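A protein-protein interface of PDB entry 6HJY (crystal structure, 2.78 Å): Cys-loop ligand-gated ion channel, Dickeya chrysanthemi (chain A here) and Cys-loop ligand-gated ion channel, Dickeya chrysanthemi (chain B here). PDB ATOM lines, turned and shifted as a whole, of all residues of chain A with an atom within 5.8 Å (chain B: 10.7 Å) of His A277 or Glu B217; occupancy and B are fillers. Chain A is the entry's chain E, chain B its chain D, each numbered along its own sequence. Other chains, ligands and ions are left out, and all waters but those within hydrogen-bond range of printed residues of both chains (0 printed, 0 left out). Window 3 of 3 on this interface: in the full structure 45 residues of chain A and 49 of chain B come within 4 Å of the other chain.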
ATOM      1  N   PHE A 221       1.732 -27.343   7.765  1.00  0.00           N
ATOM      2  CA  PHE A 221       1.341 -27.442   6.363  1.00  0.00           C
ATOM      3  C   PHE A 221       2.567 -27.332   5.442  1.00  0.00           C
ATOM      4  O   PHE A 221       2.663 -28.093   4.483  1.00  0.00           O
ATOM      5  CB  PHE A 221       0.304 -26.343   6.061  1.00  0.00           C
ATOM      6  CG  PHE A 221      -0.120 -26.141   4.624  1.00  0.00           C
ATOM      7  CD1 PHE A 221      -1.075 -26.964   4.041  1.00  0.00           C
ATOM      8  CD2 PHE A 221       0.352 -25.059   3.890  1.00  0.00           C
ATOM      9  CE1 PHE A 221      -1.509 -26.743   2.725  1.00  0.00           C
ATOM     10  CE2 PHE A 221      -0.078 -24.841   2.574  1.00  0.00           C
ATOM     11  CZ  PHE A 221      -1.018 -25.675   2.009  1.00  0.00           C
ATOM     12  N   ILE A 273      -4.254 -32.907   2.258  1.00  0.00           N
ATOM     13  CA  ILE A 273      -3.479 -31.866   2.936  1.00  0.00           C
ATOM     14  C   ILE A 273      -4.073 -30.475   2.643  1.00  0.00           C
ATOM     15  O   ILE A 273      -4.240 -29.688   3.575  1.00  0.00           O
ATOM     16  CB  ILE A 273      -1.957 -31.972   2.622  1.00  0.00           C
ATOM     17  CG1 ILE A 273      -1.341 -33.244   3.245  1.00  0.00           C
ATOM     18  CG2 ILE A 273      -1.222 -30.750   3.122  1.00  0.00           C
ATOM     19  CD1 ILE A 273      -0.013 -33.749   2.609  1.00  0.00           C
ATOM     20  N   ILE A 274      -4.416 -30.197   1.364  1.00  0.00           N
ATOM     21  CA  ILE A 274      -5.027 -28.938   0.917  1.00  0.00           C
ATOM     22  C   ILE A 274      -6.422 -28.770   1.557  1.00  0.00           C
ATOM     23  O   ILE A 274      -6.774 -27.662   1.968  1.00  0.00           O
ATOM     24  CB  ILE A 274      -5.043 -28.816  -0.646  1.00  0.00           C
ATOM     25  CG1 ILE A 274      -3.615 -28.862  -1.236  1.00  0.00           C
ATOM     26  CG2 ILE A 274      -5.787 -27.545  -1.128  1.00  0.00           C
ATOM     27  CD1 ILE A 274      -3.523 -29.313  -2.718  1.00  0.00           C
ATOM     28  N   PHE A 275      -7.172 -29.882   1.713  1.00  0.00           N
ATOM     29  CA  PHE A 275      -8.512 -29.890   2.313  1.00  0.00           C
ATOM     30  C   PHE A 275      -8.497 -29.735   3.860  1.00  0.00           C
ATOM     31  O   PHE A 275      -9.468 -30.089   4.534  1.00  0.00           O
ATOM     32  CB  PHE A 275      -9.302 -31.137   1.867  1.00  0.00           C
ATOM     33  CG  PHE A 275     -10.770 -30.879   1.606  1.00  0.00           C
ATOM     34  CD1 PHE A 275     -11.205 -30.439   0.361  1.00  0.00           C
ATOM     35  CD2 PHE A 275     -11.715 -31.078   2.602  1.00  0.00           C
ATOM     36  CE1 PHE A 275     -12.561 -30.191   0.125  1.00  0.00           C
ATOM     37  CE2 PHE A 275     -13.070 -30.825   2.367  1.00  0.00           C
ATOM     38  CZ  PHE A 275     -13.483 -30.388   1.128  1.00  0.00           C
ATOM     39  N   ALA A 276      -7.413 -29.167   4.409  1.00  0.00           N
ATOM     40  CA  ALA A 276      -7.263 -28.919   5.841  1.00  0.00           C
ATOM     41  C   ALA A 276      -6.842 -27.469   6.120  1.00  0.00           C
ATOM     42  O   ALA A 276      -7.362 -26.855   7.050  1.00  0.00           O
ATOM     43  CB  ALA A 276      -6.247 -29.885   6.428  1.00  0.00           C
ATOM     44  N   HIS A 277      -5.916 -26.927   5.301  1.00  0.00           N
ATOM     45  CA  HIS A 277      -5.368 -25.576   5.409  1.00  0.00           C
ATOM     46  C   HIS A 277      -6.368 -24.501   4.963  1.00  0.00           C
ATOM     47  O   HIS A 277      -6.946 -23.844   5.826  1.00  0.00           O
ATOM     48  CB  HIS A 277      -4.062 -25.493   4.612  1.00  0.00           C
ATOM     49  CG  HIS A 277      -3.190 -24.317   4.928  1.00  0.00           C
ATOM     50  ND1 HIS A 277      -2.554 -24.190   6.151  1.00  0.00           N
ATOM     51  CD2 HIS A 277      -2.810 -23.290   4.134  1.00  0.00           C
ATOM     52  CE1 HIS A 277      -1.851 -23.071   6.073  1.00  0.00           C
ATOM     53  NE2 HIS A 277      -1.971 -22.497   4.878  1.00  0.00           N
ATOM     54  N   HIS A 278      -6.590 -24.333   3.636  1.00  0.00           N
ATOM     55  CA  HIS A 278      -7.529 -23.342   3.096  1.00  0.00           C
ATOM     56  C   HIS A 278      -8.956 -23.900   3.001  1.00  0.00           C
ATOM     57  O   HIS A 278      -9.202 -24.892   2.314  1.00  0.00           O
ATOM     58  CB  HIS A 278      -7.059 -22.807   1.729  1.00  0.00           C
ATOM     59  CG  HIS A 278      -5.850 -21.922   1.792  1.00  0.00           C
ATOM     60  ND1 HIS A 278      -4.601 -22.378   1.413  1.00  0.00           N
ATOM     61  CD2 HIS A 278      -5.745 -20.625   2.169  1.00  0.00           C
ATOM     62  CE1 HIS A 278      -3.781 -21.353   1.567  1.00  0.00           C
ATOM     63  NE2 HIS A 278      -4.420 -20.279   2.029  1.00  0.00           N
ATOM     64  N   SER B 212      -0.058 -26.221  -7.663  1.00  0.00           N
ATOM     65  CA  SER B 212      -0.371 -26.254  -6.230  1.00  0.00           C
ATOM     66  C   SER B 212       0.647 -25.471  -5.374  1.00  0.00           C
ATOM     67  O   SER B 212       0.406 -25.274  -4.180  1.00  0.00           O
ATOM     68  CB  SER B 212      -0.512 -27.693  -5.743  1.00  0.00           C
ATOM     69  OG  SER B 212      -1.022 -27.730  -4.420  1.00  0.00           O
ATOM     70  N   VAL B 213       1.759 -25.011  -5.990  1.00  0.00           N
ATOM     71  CA  VAL B 213       2.827 -24.231  -5.346  1.00  0.00           C
ATOM     72  C   VAL B 213       2.343 -22.837  -4.915  1.00  0.00           C
ATOM     73  O   VAL B 213       2.875 -22.293  -3.948  1.00  0.00           O
ATOM     74  CB  VAL B 213       4.156 -24.161  -6.165  1.00  0.00           C
ATOM     75  CG1 VAL B 213       4.760 -25.548  -6.364  1.00  0.00           C
ATOM     76  CG2 VAL B 213       3.993 -23.435  -7.499  1.00  0.00           C
ATOM     77  N   PHE B 214       1.345 -22.268  -5.631  1.00  0.00           N
ATOM     78  CA  PHE B 214       0.765 -20.953  -5.357  1.00  0.00           C
ATOM     79  C   PHE B 214       0.000 -20.898  -4.034  1.00  0.00           C
ATOM     80  O   PHE B 214      -0.128 -19.817  -3.451  1.00  0.00           O
ATOM     81  CB  PHE B 214      -0.105 -20.468  -6.530  1.00  0.00           C
ATOM     82  CG  PHE B 214       0.685 -19.951  -7.711  1.00  0.00           C
ATOM     83  CD1 PHE B 214       1.173 -18.649  -7.727  1.00  0.00           C
ATOM     84  CD2 PHE B 214       0.937 -20.763  -8.808  1.00  0.00           C
ATOM     85  CE1 PHE B 214       1.911 -18.173  -8.818  1.00  0.00           C
ATOM     86  CE2 PHE B 214       1.671 -20.285  -9.899  1.00  0.00           C
ATOM     87  CZ  PHE B 214       2.152 -18.994  -9.896  1.00  0.00           C
ATOM     88  N   TRP B 215      -0.469 -22.068  -3.547  1.00  0.00           N
ATOM     89  CA  TRP B 215      -1.195 -22.224  -2.284  1.00  0.00           C
ATOM     90  C   TRP B 215      -0.296 -22.003  -1.058  1.00  0.00           C
ATOM     91  O   TRP B 215      -0.805 -21.902   0.061  1.00  0.00           O
ATOM     92  CB  TRP B 215      -1.896 -23.591  -2.219  1.00  0.00           C
ATOM     93  CG  TRP B 215      -3.031 -23.724  -3.189  1.00  0.00           C
ATOM     94  CD1 TRP B 215      -2.949 -24.072  -4.504  1.00  0.00           C
ATOM     95  CD2 TRP B 215      -4.422 -23.506  -2.915  1.00  0.00           C
ATOM     96  NE1 TRP B 215      -4.204 -24.089  -5.070  1.00  0.00           N
ATOM     97  CE2 TRP B 215      -5.129 -23.743  -4.118  1.00  0.00           C
ATOM     98  CE3 TRP B 215      -5.143 -23.131  -1.769  1.00  0.00           C
ATOM     99  CZ2 TRP B 215      -6.522 -23.617  -4.204  1.00  0.00           C
ATOM    100  CZ3 TRP B 215      -6.521 -23.004  -1.856  1.00  0.00           C
ATOM    101  CH2 TRP B 215      -7.198 -23.247  -3.059  1.00  0.00           C
ATOM    102  N   LEU B 216       1.039 -21.920  -1.275  1.00  0.00           N
ATOM    103  CA  LEU B 216       2.037 -21.680  -0.230  1.00  0.00           C
ATOM    104  C   LEU B 216       1.970 -20.245   0.296  1.00  0.00           C
ATOM    105  O   LEU B 216       1.596 -19.324  -0.437  1.00  0.00           O
ATOM    106  CB  LEU B 216       3.459 -22.031  -0.710  1.00  0.00           C
ATOM    107  CG  LEU B 216       3.817 -23.520  -0.747  1.00  0.00           C
ATOM    108  CD1 LEU B 216       4.961 -23.775  -1.702  1.00  0.00           C
ATOM    109  CD2 LEU B 216       4.164 -24.051   0.644  1.00  0.00           C
ATOM    110  N   GLU B 217       2.332 -20.071   1.577  1.00  0.00           N
ATOM    111  CA  GLU B 217       2.268 -18.801   2.294  1.00  0.00           C
ATOM    112  C   GLU B 217       3.352 -17.797   1.895  1.00  0.00           C
ATOM    113  O   GLU B 217       3.013 -16.675   1.507  1.00  0.00           O
ATOM    114  CB  GLU B 217       2.257 -19.025   3.825  1.00  0.00           C
ATOM    115  CG  GLU B 217       1.178 -19.977   4.337  1.00  0.00           C
ATOM    116  CD  GLU B 217      -0.250 -19.570   4.027  1.00  0.00           C
ATOM    117  OE1 GLU B 217      -0.763 -18.644   4.696  1.00  0.00           O
ATOM    118  OE2 GLU B 217      -0.852 -20.162   3.102  1.00  0.00           O
ATOM    119  N   SER B 218       4.638 -18.184   1.994  1.00  0.00           N
ATOM    120  CA  SER B 218       5.766 -17.296   1.697  1.00  0.00           C
ATOM    121  C   SER B 218       6.432 -17.526   0.336  1.00  0.00           C
ATOM    122  O   SER B 218       6.254 -18.576  -0.282  1.00  0.00           O
ATOM    123  CB  SER B 218       6.804 -17.353   2.818  1.00  0.00           C
ATOM    124  OG  SER B 218       7.560 -18.553   2.788  1.00  0.00           O
ATOM    125  N   PHE B 219       7.200 -16.509  -0.116  1.00  0.00           N
ATOM    126  CA  PHE B 219       7.963 -16.470  -1.366  1.00  0.00           C
ATOM    127  C   PHE B 219       9.096 -17.503  -1.357  1.00  0.00           C
ATOM    128  O   PHE B 219       9.371 -18.112  -2.398  1.00  0.00           O
ATOM    129  CB  PHE B 219       8.519 -15.045  -1.589  1.00  0.00           C
ATOM    130  CG  PHE B 219       9.481 -14.868  -2.745  1.00  0.00           C
ATOM    131  CD1 PHE B 219       9.013 -14.744  -4.047  1.00  0.00           C
ATOM    132  CD2 PHE B 219      10.851 -14.778  -2.525  1.00  0.00           C
ATOM    133  CE1 PHE B 219       9.902 -14.578  -5.116  1.00  0.00           C
ATOM    134  CE2 PHE B 219      11.738 -14.606  -3.596  1.00  0.00           C
ATOM    135  CZ  PHE B 219      11.256 -14.504  -4.881  1.00  0.00           C
ATOM    136  N   SER B 220       9.749 -17.692  -0.184  1.00  0.00           N
ATOM    137  CA  SER B 220      10.845 -18.649   0.044  1.00  0.00           C
ATOM    138  C   SER B 220      10.370 -20.087  -0.193  1.00  0.00           C
ATOM    139  O   SER B 220      11.116 -20.897  -0.748  1.00  0.00           O
ATOM    140  CB  SER B 220      11.405 -18.497   1.456  1.00  0.00           C
ATOM    141  OG  SER B 220      12.571 -19.276   1.664  1.00  0.00           O
ATOM    142  N   GLU B 221       9.109 -20.374   0.197  1.00  0.00           N
ATOM    143  CA  GLU B 221       8.445 -21.667   0.039  1.00  0.00           C
ATOM    144  C   GLU B 221       8.050 -21.908  -1.421  1.00  0.00           C
ATOM    145  O   GLU B 221       8.339 -22.982  -1.945  1.00  0.00           O
ATOM    146  CB  GLU B 221       7.209 -21.760   0.955  1.00  0.00           C
ATOM    147  CG  GLU B 221       7.546 -21.917   2.430  1.00  0.00           C
ATOM    148  CD  GLU B 221       6.422 -21.551   3.384  1.00  0.00           C
ATOM    149  OE1 GLU B 221       5.302 -22.091   3.232  1.00  0.00           O
ATOM    150  OE2 GLU B 221       6.673 -20.751   4.314  1.00  0.00           O
ATOM    151  N   ARG B 222       7.394 -20.908  -2.068  1.00  0.00           N
ATOM    152  CA  ARG B 222       6.912 -20.942  -3.461  1.00  0.00           C
ATOM    153  C   ARG B 222       8.015 -21.205  -4.484  1.00  0.00           C
ATOM    154  O   ARG B 222       7.797 -21.957  -5.433  1.00  0.00           O
ATOM    155  CB  ARG B 222       6.182 -19.638  -3.827  1.00  0.00           C
ATOM    156  CG  ARG B 222       4.812 -19.492  -3.195  1.00  0.00           C
ATOM    157  CD  ARG B 222       4.049 -18.367  -3.867  1.00  0.00           C
ATOM    158  NE  ARG B 222       3.164 -17.681  -2.924  1.00  0.00           N
ATOM    159  CZ  ARG B 222       3.455 -16.540  -2.306  1.00  0.00           C
ATOM    160  NH1 ARG B 222       4.620 -15.938  -2.517  1.00  0.00           N
ATOM    161  NH2 ARG B 222       2.580 -15.987  -1.475  1.00  0.00           N
ATOM    162  N   LEU B 223       9.182 -20.565  -4.306  1.00  0.00           N
ATOM    163  CA  LEU B 223      10.321 -20.682  -5.216  1.00  0.00           C
ATOM    164  C   LEU B 223      11.045 -22.030  -5.075  1.00  0.00           C
ATOM    165  O   LEU B 223      11.224 -22.713  -6.084  1.00  0.00           O
ATOM    166  CB  LEU B 223      11.269 -19.484  -5.020  1.00  0.00           C
ATOM    167  CG  LEU B 223      12.492 -19.365  -5.935  1.00  0.00           C
ATOM    168  CD1 LEU B 223      12.703 -17.920  -6.346  1.00  0.00           C
ATOM    169  CD2 LEU B 223      13.748 -19.829  -5.216  1.00  0.00           C
ATOM    170  N   THR B 225      10.037 -24.856  -3.974  1.00  0.00           N
ATOM    171  CA  THR B 225       9.160 -25.956  -4.390  1.00  0.00           C
ATOM    172  C   THR B 225       9.062 -26.006  -5.926  1.00  0.00           C
ATOM    173  O   THR B 225       8.915 -27.094  -6.487  1.00  0.00           O
ATOM    174  CB  THR B 225       7.806 -25.888  -3.658  1.00  0.00           C
ATOM    175  OG1 THR B 225       8.032 -25.653  -2.268  1.00  0.00           O
ATOM    176  CG2 THR B 225       6.995 -27.168  -3.803  1.00  0.00           C
ATOM    177  N   ILE B 271       5.835 -15.874  -9.984  1.00  0.00           N
ATOM    178  CA  ILE B 271       6.294 -15.706  -8.601  1.00  0.00           C
ATOM    179  C   ILE B 271       7.266 -14.510  -8.507  1.00  0.00           C
ATOM    180  O   ILE B 271       7.147 -13.714  -7.573  1.00  0.00           O
ATOM    181  CB  ILE B 271       6.848 -17.039  -7.992  1.00  0.00           C
ATOM    182  CG1 ILE B 271       5.750 -18.132  -7.960  1.00  0.00           C
ATOM    183  CG2 ILE B 271       7.425 -16.838  -6.581  1.00  0.00           C
ATOM    184  CD1 ILE B 271       6.259 -19.596  -7.944  1.00  0.00           C
ATOM    185  N   ALA B 274       5.908 -10.709  -8.536  1.00  0.00           N
ATOM    186  CA  ALA B 274       5.155 -10.362  -7.332  1.00  0.00           C
ATOM    187  C   ALA B 274       6.075  -9.730  -6.278  1.00  0.00           C
ATOM    188  O   ALA B 274       5.689  -8.746  -5.647  1.00  0.00           O
ATOM    189  CB  ALA B 274       4.485 -11.606  -6.766  1.00  0.00           C
ATOM    190  N   HIS B 275       7.297 -10.291  -6.114  1.00  0.00           N
ATOM    191  CA  HIS B 275       8.319  -9.863  -5.157  1.00  0.00           C
ATOM    192  C   HIS B 275       8.995  -8.548  -5.574  1.00  0.00           C
ATOM    193  O   HIS B 275       8.650  -7.506  -5.017  1.00  0.00           O
ATOM    194  CB  HIS B 275       9.340 -10.999  -4.939  1.00  0.00           C
ATOM    195  CG  HIS B 275      10.165 -10.868  -3.694  1.00  0.00           C
ATOM    196  ND1 HIS B 275       9.615 -11.039  -2.436  1.00  0.00           N
ATOM    197  CD2 HIS B 275      11.493 -10.647  -3.565  1.00  0.00           C
ATOM    198  CE1 HIS B 275      10.612 -10.881  -1.586  1.00  0.00           C
ATOM    199  NE2 HIS B 275      11.764 -10.645  -2.215  1.00  0.00           N
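A ring nitrogen (NE2) of His A277 sits at hydrogen-bond distance from the side-chain carboxylate (OE2) of Glu B217, 3.1 Å away.
The backbone carbonyl oxygen (O) of Glu B217 lies within hydrogen-bond range of the guanidinium group (NH2) of Arg B222 (3.1 Å).
O of Trp B215 touches CE2 of Phe A221, at 3.9 Å. Ser B212 touches Ile A274. His A278 touches Trp B215. Glu B217 touches His A278 (OE2 to CE1, 3.5 Å).
Of the printed residues of chain B, Phe A221 touches Trp B215 (3.9 Å). Of the printed residues of chain B, Ile A274 touches Ser B212. No residue of chain B comes within 4 Å of Ala A276. His A277 touches just one residue of chain B: Glu B217. Of the printed residues of chain A, Ser B212 touches Ile A274. Of the printed residues of chain A, Trp B215 touches Phe A221 and His A278. Glu B217 touches just these residues of chain A: His A277 and His A278.
Of the 7 printed residues of chain A, 4 touch a printed residue of chain B. Printed residues of chain B that touch a printed residue of chain A: Ser B212, Trp B215 and Glu B217. Hydrophobic or aromatic side chains of chain B within 4 Å of the printed part of chain A: Trp B215. Among the printed residues, no Asp or Glu carboxylate lies within 4 Å of a Lys or Arg side-chain nitrogen of the other chain.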
